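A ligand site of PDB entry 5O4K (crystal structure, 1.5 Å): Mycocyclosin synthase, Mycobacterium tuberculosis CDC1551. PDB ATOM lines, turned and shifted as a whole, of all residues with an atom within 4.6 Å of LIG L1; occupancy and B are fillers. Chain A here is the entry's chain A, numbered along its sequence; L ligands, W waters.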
ATOM      1  N   MET A  62      -5.444  -0.588   5.599  1.00  0.00           N
ATOM      2  CA  MET A  62      -5.392  -1.687   4.600  1.00  0.00           C
ATOM      3  C   MET A  62      -6.358  -2.784   4.992  1.00  0.00           C
ATOM      4  O   MET A  62      -7.144  -3.266   4.160  1.00  0.00           O
ATOM      5  CB  MET A  62      -3.979  -2.341   4.422  1.00  0.00           C
ATOM      6  CG  MET A  62      -3.975  -3.737   3.735  1.00  0.00           C
ATOM      7  SD  MET A  62      -2.314  -4.352   3.392  1.00  0.00           S
ATOM      8  CE  MET A  62      -1.524  -3.009   2.556  1.00  0.00           C
ATOM      9  N   MET A  86       0.756  -9.201   6.716  1.00  0.00           N
ATOM     10  CA  MET A  86       1.900  -8.794   7.526  1.00  0.00           C
ATOM     11  C   MET A  86       1.532  -8.491   8.946  1.00  0.00           C
ATOM     12  O   MET A  86       2.263  -8.816   9.894  1.00  0.00           O
ATOM     13  CB  MET A  86       2.626  -7.628   6.872  1.00  0.00           C
ATOM     14  CG  MET A  86       3.513  -8.141   5.810  1.00  0.00           C
ATOM     15  SD  MET A  86       5.125  -8.710   6.313  1.00  0.00           S
ATOM     16  CE  MET A  86       5.424  -8.436   8.053  1.00  0.00           C
ATOM     17  N   ARG A  95       7.715 -11.517  12.473  1.00  0.00           N
ATOM     18  CA  ARG A  95       8.197 -10.436  11.570  1.00  0.00           C
ATOM     19  C   ARG A  95       9.724 -10.434  11.365  1.00  0.00           C
ATOM     20  O   ARG A  95      10.243 -10.423  10.241  1.00  0.00           O
ATOM     21  CB  ARG A  95       7.688  -9.069  12.084  1.00  0.00           C
ATOM     22  CG  ARG A  95       8.014  -7.907  11.155  1.00  0.00           C
ATOM     23  CD  ARG A  95       7.430  -6.557  11.595  1.00  0.00           C
ATOM     24  NE  ARG A  95       7.479  -5.698  10.424  1.00  0.00           N
ATOM     25  CZ  ARG A  95       6.452  -5.289   9.666  1.00  0.00           C
ATOM     26  NH1 ARG A  95       5.166  -5.512   9.999  1.00  0.00           N
ATOM     27  NH2 ARG A  95       6.738  -4.561   8.561  1.00  0.00           N
ATOM     28  N   ILE A 102      14.343 -12.792   3.859  1.00  0.00           N
ATOM     29  CA  ILE A 102      14.077 -12.262   2.524  1.00  0.00           C
ATOM     30  C   ILE A 102      15.036 -11.131   2.169  1.00  0.00           C
ATOM     31  O   ILE A 102      14.772 -10.429   1.163  1.00  0.00           O
ATOM     32  CB  ILE A 102      12.604 -11.875   2.290  1.00  0.00           C
ATOM     33  CG1 ILE A 102      12.174 -10.687   3.146  1.00  0.00           C
ATOM     34  CG2 ILE A 102      11.673 -13.069   2.476  1.00  0.00           C
ATOM     35  CD1 ILE A 102      10.812 -10.194   2.818  1.00  0.00           C
ATOM     36  N   HIS A 146      12.968 -16.631  -6.003  1.00  0.00           N
ATOM     37  CA  HIS A 146      12.031 -16.871  -4.904  1.00  0.00           C
ATOM     38  C   HIS A 146      12.054 -18.322  -4.450  1.00  0.00           C
ATOM     39  O   HIS A 146      11.847 -18.590  -3.248  1.00  0.00           O
ATOM     40  CB  HIS A 146      10.670 -16.302  -5.193  1.00  0.00           C
ATOM     41  CG  HIS A 146      10.658 -14.826  -5.081  1.00  0.00           C
ATOM     42  ND1 HIS A 146      11.184 -14.020  -6.087  1.00  0.00           N
ATOM     43  CD2 HIS A 146      10.349 -14.010  -4.049  1.00  0.00           C
ATOM     44  CE1 HIS A 146      11.120 -12.751  -5.658  1.00  0.00           C
ATOM     45  NE2 HIS A 146      10.628 -12.715  -4.432  1.00  0.00           N
ATOM     46  N   PHE A 230       4.399 -14.849   0.103  1.00  0.00           N
ATOM     47  CA  PHE A 230       5.715 -14.274  -0.190  1.00  0.00           C
ATOM     48  C   PHE A 230       6.202 -14.738  -1.550  1.00  0.00           C
ATOM     49  O   PHE A 230       6.777 -13.927  -2.293  1.00  0.00           O
ATOM     50  CB  PHE A 230       6.707 -14.496   0.974  1.00  0.00           C
ATOM     51  CG  PHE A 230       6.555 -13.437   2.041  1.00  0.00           C
ATOM     52  CD1 PHE A 230       5.367 -13.311   2.798  1.00  0.00           C
ATOM     53  CD2 PHE A 230       7.533 -12.456   2.196  1.00  0.00           C
ATOM     54  CE1 PHE A 230       5.184 -12.298   3.750  1.00  0.00           C
ATOM     55  CE2 PHE A 230       7.335 -11.441   3.131  1.00  0.00           C
ATOM     56  CZ  PHE A 230       6.207 -11.369   3.883  1.00  0.00           C
ATOM     57  N   ALA A 233       3.712 -12.682  -4.149  1.00  0.00           N
ATOM     58  CA  ALA A 233       3.942 -11.246  -4.097  1.00  0.00           C
ATOM     59  C   ALA A 233       5.338 -10.903  -4.613  1.00  0.00           C
ATOM     60  O   ALA A 233       5.503  -9.987  -5.433  1.00  0.00           O
ATOM     61  CB  ALA A 233       3.801 -10.781  -2.669  1.00  0.00           C
ATOM     62  N   GLY A 234       6.354 -11.681  -4.229  1.00  0.00           N
ATOM     63  CA  GLY A 234       7.680 -11.354  -4.624  1.00  0.00           C
ATOM     64  C   GLY A 234       7.876 -11.643  -6.102  1.00  0.00           C
ATOM     65  O   GLY A 234       8.491 -10.824  -6.812  1.00  0.00           O
ATOM     66  N   SER A 237       5.946  -9.176  -8.400  1.00  0.00           N
ATOM     67  CA  SER A 237       6.403  -7.819  -8.288  1.00  0.00           C
ATOM     68  C   SER A 237       7.787  -7.640  -8.933  1.00  0.00           C
ATOM     69  O   SER A 237       8.022  -6.649  -9.670  1.00  0.00           O
ATOM     70  CB  SER A 237       6.410  -7.306  -6.823  1.00  0.00           C
ATOM     71  OG  SER A 237       5.094  -7.345  -6.320  1.00  0.00           O
ATOM     72  N   THR A 238       8.723  -8.515  -8.630  1.00  0.00           N
ATOM     73  CA  THR A 238      10.075  -8.424  -9.185  1.00  0.00           C
ATOM     74  C   THR A 238      10.079  -8.773 -10.656  1.00  0.00           C
ATOM     75  O   THR A 238      10.785  -8.073 -11.459  1.00  0.00           O
ATOM     76  CB  THR A 238      11.076  -9.330  -8.449  1.00  0.00           C
ATOM     77  OG1 THR A 238      10.690 -10.679  -8.503  1.00  0.00           O
ATOM     78  CG2 THR A 238      11.272  -8.867  -7.004  1.00  0.00           C
ATOM     79  N   PHE A 241       8.320  -5.680 -12.371  1.00  0.00           N
ATOM     80  CA  PHE A 241       9.152  -4.490 -12.335  1.00  0.00           C
ATOM     81  C   PHE A 241      10.357  -4.608 -13.263  1.00  0.00           C
ATOM     82  O   PHE A 241      10.651  -3.675 -14.051  1.00  0.00           O
ATOM     83  CB  PHE A 241       9.647  -4.149 -10.905  1.00  0.00           C
ATOM     84  CG  PHE A 241      10.694  -3.098 -10.894  1.00  0.00           C
ATOM     85  CD1 PHE A 241      10.355  -1.830 -11.334  1.00  0.00           C
ATOM     86  CD2 PHE A 241      12.032  -3.335 -10.593  1.00  0.00           C
ATOM     87  CE1 PHE A 241      11.316  -0.863 -11.484  1.00  0.00           C
ATOM     88  CE2 PHE A 241      12.988  -2.360 -10.733  1.00  0.00           C
ATOM     89  CZ  PHE A 241      12.625  -1.129 -11.215  1.00  0.00           C
ATOM     90  N   LEU A 274      12.823   2.531 -10.650  1.00  0.00           N
ATOM     91  CA  LEU A 274      11.780   2.356  -9.634  1.00  0.00           C
ATOM     92  C   LEU A 274      10.885   3.575  -9.576  1.00  0.00           C
ATOM     93  O   LEU A 274       9.669   3.468  -9.615  1.00  0.00           O
ATOM     94  CB  LEU A 274      12.412   2.095  -8.236  1.00  0.00           C
ATOM     95  CG  LEU A 274      12.854   0.639  -8.089  1.00  0.00           C
ATOM     96  CD1 LEU A 274      13.819   0.515  -6.919  1.00  0.00           C
ATOM     97  CD2 LEU A 274      11.704  -0.322  -7.894  1.00  0.00           C
ATOM     98  N   PHE A 280       2.520  -0.940 -10.976  1.00  0.00           N
ATOM     99  CA  PHE A 280       1.229  -1.059 -10.273  1.00  0.00           C
ATOM    100  C   PHE A 280       0.126  -0.506 -11.085  1.00  0.00           C
ATOM    101  O   PHE A 280       0.084   0.658 -11.401  1.00  0.00           O
ATOM    102  CB  PHE A 280       1.237  -0.415  -8.861  1.00  0.00           C
ATOM    103  CG  PHE A 280       1.845  -1.286  -7.802  1.00  0.00           C
ATOM    104  CD1 PHE A 280       3.160  -1.701  -7.877  1.00  0.00           C
ATOM    105  CD2 PHE A 280       1.064  -1.759  -6.740  1.00  0.00           C
ATOM    106  CE1 PHE A 280       3.723  -2.535  -6.888  1.00  0.00           C
ATOM    107  CE2 PHE A 280       1.621  -2.566  -5.738  1.00  0.00           C
ATOM    108  CZ  PHE A 280       2.935  -2.983  -5.859  1.00  0.00           C
ATOM    109  N   LEU A 284      -3.023   2.147  -4.587  1.00  0.00           N
ATOM    110  CA  LEU A 284      -3.049   1.335  -3.373  1.00  0.00           C
ATOM    111  C   LEU A 284      -4.326   1.650  -2.576  1.00  0.00           C
ATOM    112  O   LEU A 284      -4.596   2.807  -2.270  1.00  0.00           O
ATOM    113  CB  LEU A 284      -1.842   1.596  -2.504  1.00  0.00           C
ATOM    114  CG  LEU A 284      -0.458   1.438  -3.139  1.00  0.00           C
ATOM    115  CD1 LEU A 284       0.600   1.761  -2.104  1.00  0.00           C
ATOM    116  CD2 LEU A 284      -0.326   0.027  -3.722  1.00  0.00           C
ATOM    117  N   ARG A 286      -7.068   1.892   0.478  1.00  0.00           N
ATOM    118  CA  ARG A 286      -7.227   2.067   1.929  1.00  0.00           C
ATOM    119  C   ARG A 286      -8.656   2.417   2.218  1.00  0.00           C
ATOM    120  O   ARG A 286      -9.351   3.068   1.411  1.00  0.00           O
ATOM    121  CB  ARG A 286      -6.383   3.231   2.395  1.00  0.00           C
ATOM    122  CG  ARG A 286      -4.865   3.045   2.284  1.00  0.00           C
ATOM    123  CD  ARG A 286      -4.366   1.991   3.208  1.00  0.00           C
ATOM    124  NE  ARG A 286      -2.882   1.923   3.229  1.00  0.00           N
ATOM    125  CZ  ARG A 286      -2.137   1.147   2.463  1.00  0.00           C
ATOM    126  NH1 ARG A 286      -2.640   0.418   1.494  1.00  0.00           N
ATOM    127  NH2 ARG A 286      -0.805   1.176   2.678  1.00  0.00           N
ATOM    128  N   LEU A 309       0.483   5.657  -7.188  1.00  0.00           N
ATOM    129  CA  LEU A 309       1.933   5.761  -6.990  1.00  0.00           C
ATOM    130  C   LEU A 309       2.588   6.629  -8.056  1.00  0.00           C
ATOM    131  O   LEU A 309       3.485   7.462  -7.710  1.00  0.00           O
ATOM    132  CB  LEU A 309       2.555   4.398  -6.940  1.00  0.00           C
ATOM    133  CG  LEU A 309       2.106   3.543  -5.771  1.00  0.00           C
ATOM    134  CD1 LEU A 309       2.823   2.209  -5.849  1.00  0.00           C
ATOM    135  CD2 LEU A 309       2.273   4.169  -4.409  1.00  0.00           C
ATOM    136  N   LEU A 336       7.798   6.572  -3.940  1.00  0.00           N
ATOM    137  CA  LEU A 336       6.835   5.689  -3.288  1.00  0.00           C
ATOM    138  C   LEU A 336       6.696   4.328  -3.959  1.00  0.00           C
ATOM    139  O   LEU A 336       5.688   3.628  -3.790  1.00  0.00           O
ATOM    140  CB  LEU A 336       5.476   6.392  -3.199  1.00  0.00           C
ATOM    141  CG  LEU A 336       5.455   7.772  -2.546  1.00  0.00           C
ATOM    142  CD1 LEU A 336       4.002   8.188  -2.300  1.00  0.00           C
ATOM    143  CD2 LEU A 336       6.222   7.848  -1.274  1.00  0.00           C
ATOM    144  N   ALA A 337       7.681   3.926  -4.770  1.00  0.00           N
ATOM    145  CA  ALA A 337       7.577   2.630  -5.444  1.00  0.00           C
ATOM    146  C   ALA A 337       7.434   1.429  -4.547  1.00  0.00           C
ATOM    147  O   ALA A 337       6.805   0.463  -4.981  1.00  0.00           O
ATOM    148  CB  ALA A 337       8.771   2.391  -6.392  1.00  0.00           C
ATOM    149  N   PHE A 338       7.934   1.514  -3.301  1.00  0.00           N
ATOM    150  CA  PHE A 338       7.783   0.449  -2.301  1.00  0.00           C
ATOM    151  C   PHE A 338       6.773   0.835  -1.212  1.00  0.00           C
ATOM    152  O   PHE A 338       6.732   0.235  -0.132  1.00  0.00           O
ATOM    153  CB  PHE A 338       9.109   0.157  -1.656  1.00  0.00           C
ATOM    154  CG  PHE A 338      10.132  -0.460  -2.627  1.00  0.00           C
ATOM    155  CD1 PHE A 338       9.896  -1.697  -3.173  1.00  0.00           C
ATOM    156  CD2 PHE A 338      11.333   0.144  -2.914  1.00  0.00           C
ATOM    157  CE1 PHE A 338      10.804  -2.282  -4.025  1.00  0.00           C
ATOM    158  CE2 PHE A 338      12.263  -0.452  -3.745  1.00  0.00           C
ATOM    159  CZ  PHE A 338      11.996  -1.678  -4.316  1.00  0.00           C
ATOM    160  N   GLY A 339       5.957   1.832  -1.511  1.00  0.00           N
ATOM    161  CA  GLY A 339       5.033   2.352  -0.510  1.00  0.00           C
ATOM    162  C   GLY A 339       5.696   3.253   0.493  1.00  0.00           C
ATOM    163  O   GLY A 339       6.790   3.803   0.290  1.00  0.00           O
ATOM    164  N   GLN A 342       3.355   2.224   7.489  1.00  0.00           N
ATOM    165  CA  GLN A 342       3.182   0.904   8.156  1.00  0.00           C
ATOM    166  C   GLN A 342       3.371  -0.260   7.198  1.00  0.00           C
ATOM    167  O   GLN A 342       3.933  -1.278   7.606  1.00  0.00           O
ATOM    168  CB  GLN A 342       1.759   0.802   8.741  1.00  0.00           C
ATOM    169  CG  GLN A 342       1.358  -0.521   9.420  1.00  0.00           C
ATOM    170  CD  GLN A 342       2.020  -0.716  10.733  1.00  0.00           C
ATOM    171  OE1 GLN A 342       2.621   0.208  11.292  1.00  0.00           O
ATOM    172  NE2 GLN A 342       1.904  -1.930  11.280  1.00  0.00           N
ATOM    173  N   HIS A 343       2.987  -0.108   5.933  1.00  0.00           N
ATOM    174  CA  HIS A 343       2.972  -1.204   5.003  1.00  0.00           C
ATOM    175  C   HIS A 343       4.086  -1.170   3.959  1.00  0.00           C
ATOM    176  O   HIS A 343       3.985  -1.871   2.920  1.00  0.00           O
ATOM    177  CB  HIS A 343       1.582  -1.281   4.343  1.00  0.00           C
ATOM    178  CG  HIS A 343       0.511  -1.685   5.310  1.00  0.00           C
ATOM    179  ND1 HIS A 343      -0.367  -0.790   5.888  1.00  0.00           N
ATOM    180  CD2 HIS A 343       0.247  -2.891   5.842  1.00  0.00           C
ATOM    181  CE1 HIS A 343      -1.157  -1.462   6.724  1.00  0.00           C
ATOM    182  NE2 HIS A 343      -0.783  -2.723   6.753  1.00  0.00           N
ATOM    183  N   PHE A 344       5.127  -0.389   4.263  1.00  0.00           N
ATOM    184  CA  PHE A 344       6.327  -0.302   3.385  1.00  0.00           C
ATOM    185  C   PHE A 344       6.819  -1.728   3.043  1.00  0.00           C
ATOM    186  O   PHE A 344       6.907  -2.618   3.913  1.00  0.00           O
ATOM    187  CB  PHE A 344       7.433   0.458   4.056  1.00  0.00           C
ATOM    188  CG  PHE A 344       8.646   0.642   3.215  1.00  0.00           C
ATOM    189  CD1 PHE A 344       8.697   1.673   2.306  1.00  0.00           C
ATOM    190  CD2 PHE A 344       9.715  -0.226   3.290  1.00  0.00           C
ATOM    191  CE1 PHE A 344       9.815   1.863   1.499  1.00  0.00           C
ATOM    192  CE2 PHE A 344      10.785  -0.054   2.445  1.00  0.00           C
ATOM    193  CZ  PHE A 344      10.816   0.952   1.555  1.00  0.00           C
ATOM    194  N   CYS A 345       7.138  -1.932   1.744  1.00  0.00           N
ATOM    195  CA  CYS A 345       7.501  -3.271   1.232  1.00  0.00           C
ATOM    196  C   CYS A 345       8.655  -3.939   2.034  1.00  0.00           C
ATOM    197  O   CYS A 345       9.785  -3.393   2.074  1.00  0.00           O
ATOM    198  CB  CYS A 345       7.945  -3.138  -0.198  1.00  0.00           C
ATOM    199  SG  CYS A 345       8.279  -4.749  -0.938  1.00  0.00           S
ATOM    200  N   PRO A 346       8.406  -5.119   2.601  1.00  0.00           N
ATOM    201  CA  PRO A 346       9.505  -5.816   3.291  1.00  0.00           C
ATOM    202  C   PRO A 346      10.525  -6.447   2.349  1.00  0.00           C
ATOM    203  O   PRO A 346      11.650  -6.859   2.793  1.00  0.00           O
ATOM    204  CB  PRO A 346       8.740  -6.893   4.068  1.00  0.00           C
ATOM    205  CG  PRO A 346       7.559  -7.195   3.283  1.00  0.00           C
ATOM    206  CD  PRO A 346       7.128  -5.861   2.687  1.00  0.00           C
ATOM    207  N   GLY A 347      10.162  -6.525   1.071  1.00  0.00           N
ATOM    208  CA  GLY A 347      11.034  -7.116   0.042  1.00  0.00           C
ATOM    209  C   GLY A 347      11.856  -6.067  -0.713  1.00  0.00           C
ATOM    210  O   GLY A 347      12.413  -6.368  -1.769  1.00  0.00           O
ATOM    211  N   LEU A 350      15.507  -6.929  -1.604  1.00  0.00           N
ATOM    212  CA  LEU A 350      15.562  -8.058  -2.541  1.00  0.00           C
ATOM    213  C   LEU A 350      15.147  -7.621  -3.956  1.00  0.00           C
ATOM    214  O   LEU A 350      15.744  -8.060  -4.952  1.00  0.00           O
ATOM    215  CB  LEU A 350      14.676  -9.144  -2.039  1.00  0.00           C
ATOM    216  CG  LEU A 350      14.765 -10.489  -2.743  1.00  0.00           C
ATOM    217  CD1 LEU A 350      16.133 -11.098  -2.650  1.00  0.00           C
ATOM    218  CD2 LEU A 350      13.715 -11.454  -2.206  1.00  0.00           C
ATOM    219  N   GLY A 351      14.101  -6.809  -4.053  1.00  0.00           N
ATOM    220  CA  GLY A 351      13.650  -6.319  -5.306  1.00  0.00           C
ATOM    221  C   GLY A 351      14.652  -5.417  -5.991  1.00  0.00           C
ATOM    222  O   GLY A 351      14.895  -5.577  -7.228  1.00  0.00           O
HETATM  223  C1  LIG L   1       4.153  -4.184   0.137  1.00  0.00           C
HETATM  224  C2  LIG L   1       6.033  -2.763  -4.121  1.00  0.00           C
HETATM  225  C3  LIG L   1       8.889  -6.693  -4.064  1.00  0.00           C
HETATM  226  C4  LIG L   1       6.293  -8.536  -0.467  1.00  0.00           C
HETATM  227  C5  LIG L   1       4.497  -3.399  -0.973  1.00  0.00           C
HETATM  228  C6  LIG L   1       3.926  -2.096  -1.260  1.00  0.00           C
HETATM  229  C7  LIG L   1       4.417  -1.738  -2.475  1.00  0.00           C
HETATM  230  C8  LIG L   1       5.314  -2.742  -2.930  1.00  0.00           C
HETATM  231  C9  LIG L   1       4.102  -0.496  -3.260  1.00  0.00           C
HETATM  232  C10 LIG L   1       2.946  -1.363  -0.358  1.00  0.00           C
HETATM  233  C11 LIG L   1       1.525  -1.830  -0.558  1.00  0.00           C
HETATM  234  C12 LIG L   1       0.556  -0.970   0.252  1.00  0.00           C
HETATM  235  O1  LIG L   1       0.966  -0.158   1.091  1.00  0.00           O
HETATM  236  O2  LIG L   1      -0.703  -1.192   0.010  1.00  0.00           O
HETATM  237  C13 LIG L   1       6.971  -3.720  -4.524  1.00  0.00           C
HETATM  238  C14 LIG L   1       7.805  -3.614  -5.679  1.00  0.00           C
HETATM  239  C15 LIG L   1       8.622  -4.712  -5.649  1.00  0.00           C
HETATM  240  C16 LIG L   1       8.278  -5.497  -4.471  1.00  0.00           C
HETATM  241  C17 LIG L   1       7.811  -2.485  -6.658  1.00  0.00           C
HETATM  242  C18 LIG L   1       9.746  -5.077  -6.542  1.00  0.00           C
HETATM  243  C19 LIG L   1      10.468  -4.246  -7.266  1.00  0.00           C
HETATM  244  C20 LIG L   1       8.471  -7.548  -3.072  1.00  0.00           C
HETATM  245  C21 LIG L   1       9.138  -8.769  -2.733  1.00  0.00           C
HETATM  246  C22 LIG L   1       8.305  -9.269  -1.725  1.00  0.00           C
HETATM  247  C23 LIG L   1       7.274  -8.375  -1.426  1.00  0.00           C
HETATM  248  C24 LIG L   1      10.391  -9.351  -3.336  1.00  0.00           C
HETATM  249  C25 LIG L   1       8.451 -10.540  -0.983  1.00  0.00           C
HETATM  250  C26 LIG L   1       9.335 -11.493  -1.253  1.00  0.00           C
HETATM  251  C27 LIG L   1       5.468  -7.489  -0.048  1.00  0.00           C
HETATM  252  C28 LIG L   1       4.569  -7.621   1.104  1.00  0.00           C
HETATM  253  C29 LIG L   1       3.968  -6.419   1.314  1.00  0.00           C
HETATM  254  C30 LIG L   1       4.512  -5.520   0.245  1.00  0.00           C
HETATM  255  C31 LIG L   1       4.363  -8.911   1.885  1.00  0.00           C
HETATM  256  C32 LIG L   1       2.946  -6.000   2.381  1.00  0.00           C
HETATM  257  C33 LIG L   1       3.594  -5.334   3.579  1.00  0.00           C
HETATM  258  C34 LIG L   1       2.659  -4.882   4.740  1.00  0.00           C
HETATM  259  O3  LIG L   1       3.185  -4.397   5.785  1.00  0.00           O
HETATM  260  O4  LIG L   1       1.470  -4.946   4.441  1.00  0.00           O
HETATM  261  N1  LIG L   1       5.372  -3.788  -1.993  1.00  0.00           N
HETATM  262  N2  LIG L   1       7.268  -4.870  -3.820  1.00  0.00           N
HETATM  263  N3  LIG L   1       7.415  -7.295  -2.270  1.00  0.00           N
HETATM  264  N4  LIG L   1       5.480  -6.177  -0.501  1.00  0.00           N
HETATM  265 FE1  LIG L   1       6.390  -5.505  -2.103  1.00  0.00          FE
HETATM  266  C1  LG2 L   2       4.493  -7.424  -3.508  1.00  0.00           C
HETATM  267  C2  LG2 L   2      -1.139  -7.070  -0.814  1.00  0.00           C
HETATM  268  C3  LG2 L   2      -1.394 -11.644  -0.709  1.00  0.00           C
HETATM  269  C4  LG2 L   2      -0.724 -13.501  -2.668  1.00  0.00           C
HETATM  270  C5  LG2 L   2      -2.020 -13.422  -2.256  1.00  0.00           C
HETATM  271  O1  LG2 L   2       0.719  -9.914   1.509  1.00  0.00           O
HETATM  272  C6  LG2 L   2       0.193  -9.145   0.763  1.00  0.00           C
HETATM  273  C7  LG2 L   2       0.808  -7.755   0.372  1.00  0.00           C
HETATM  274  N1  LG2 L   2       0.332  -7.143  -0.902  1.00  0.00           N
HETATM  275  C8  LG2 L   2       0.877  -5.757  -0.989  1.00  0.00           C
HETATM  276  C9  LG2 L   2       0.654  -5.162  -2.392  1.00  0.00           C
HETATM  277  C10 LG2 L   2       1.129  -6.084  -3.488  1.00  0.00           C
HETATM  278  N2  LG2 L   2       2.522  -6.370  -3.432  1.00  0.00           N
HETATM  279  C11 LG2 L   2       3.107  -7.591  -3.721  1.00  0.00           C
HETATM  280  N3  LG2 L   2       4.761  -6.206  -3.142  1.00  0.00           N
HETATM  281  C12 LG2 L   2       3.562  -5.582  -3.104  1.00  0.00           C
HETATM  282  C13 LG2 L   2      -1.732  -8.417  -0.810  1.00  0.00           C
HETATM  283  N4  LG2 L   2      -1.123  -9.390   0.116  1.00  0.00           N
HETATM  284  C14 LG2 L   2      -1.737 -10.651   0.342  1.00  0.00           C
HETATM  285  C15 LG2 L   2      -0.075 -11.778  -1.212  1.00  0.00           C
HETATM  286  C16 LG2 L   2       0.243 -12.686  -2.168  1.00  0.00           C
HETATM  287 CL1  LG2 L   2      -0.299 -14.692  -3.833  1.00  0.00          CL
HETATM  288  C17 LG2 L   2      -2.335 -12.489  -1.260  1.00  0.00           C
HETATM  289  O   HOH W   1      -2.060  -2.891  -1.504  1.00  0.00           O
HETATM  290  O   HOH W   2       2.905   1.454   2.013  1.00  0.00           O
HETATM  291  O   HOH W   3       2.717  -4.026   8.335  1.00  0.00           O
HETATM  292  O   HOH W   4       5.792  -3.974   6.069  1.00  0.00           O
HETATM  293  O   HOH W   5       0.015  -7.254   4.553  1.00  0.00           O
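An iron atom (FE1) of LIG L1 is bound by the side-chain sulfur (SG) of Cys 345 (2.3 Å).
An oxygen (O1) of LIG L1 lies within salt-bridge range of the guanidinium group (NH2) of Arg 286, 2.7 Å away.
OG of Ser 237 sits close to N3 of LG2 L2 (3.4 Å).
N3 of LG2 L2 is bound to FE1 of LIG L1 (2.1 Å).
The backbone NH (N) of Cys 345 sits at hydrogen-bond distance from the backbone carbonyl oxygen (O) of Phe 338 (2.9 Å).
The side-chain sulfur (SG) of Cys 345 sits close to the backbone NH (N) of Gly 347 (3.3 Å).
OG of Ser 237 lies within hydrogen-bond range of O of Ala 233 (2.8 Å).
The backbone carbonyl oxygen (O) of Gly 234 sits at hydrogen-bond distance from the side-chain hydroxyl (OG1) of Thr 238 (2.8 Å).
Residues that only touch LIG L1: Met 62 (3.2 Å), Met 86 (3.5 Å), His 146 (3.5 Å), Phe 230 (3.7 Å), Gly 234 (3.5 Å), Ser 237 (3.5 Å), Thr 238 (3.8 Å), Phe 241 (3.7 Å), Phe 280 (3.6 Å), Leu 284 (3.6 Å), Leu 309 (3.96 Å), Ala 337 (3.3 Å), Phe 338 (3.6 Å), Gly 339 (3.5 Å), Gln 342 (3.7 Å), His 343 (2.8 Å), Pro 346 (3.5 Å) and Gly 347 (3.7 Å).
Hydrophobic or aromatic side chains that line LIG L1: Met 62, Met 86, His 146, Phe 230, Phe 241, Phe 280, Leu 284, Leu 309, Phe 338, His 343 and Pro 346.
Within 4 Å of LIG L1: Met 62, Met 86, His 146, Phe 230, Gly 234, Ser 237, Thr 238, Phe 241, Phe 280, Leu 284, Arg 286, Leu 309, Ala 337, Phe 338, Gly 339, Gln 342, His 343, Cys 345, Pro 346 and Gly 347.
Water W3 lies within hydrogen-bond range of an oxygen (O3) of LIG L1 (2.6 Å), the backbone carbonyl oxygen (O) of Gln 342 (3.1 Å) and the guanidinium group (NH1) of Arg 95 (3.3 Å).
Water W4 lies within hydrogen-bond range of an oxygen (O3) of LIG L1 (2.7 Å), the guanidinium group (NH2) of Arg 95 (2.7 Å) and the backbone carbonyl oxygen (O) of Phe 344 (2.8 Å).
Water W5 bridges O4 of LIG L1 (2.7 Å) and N of Met 86 (3.0 Å).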
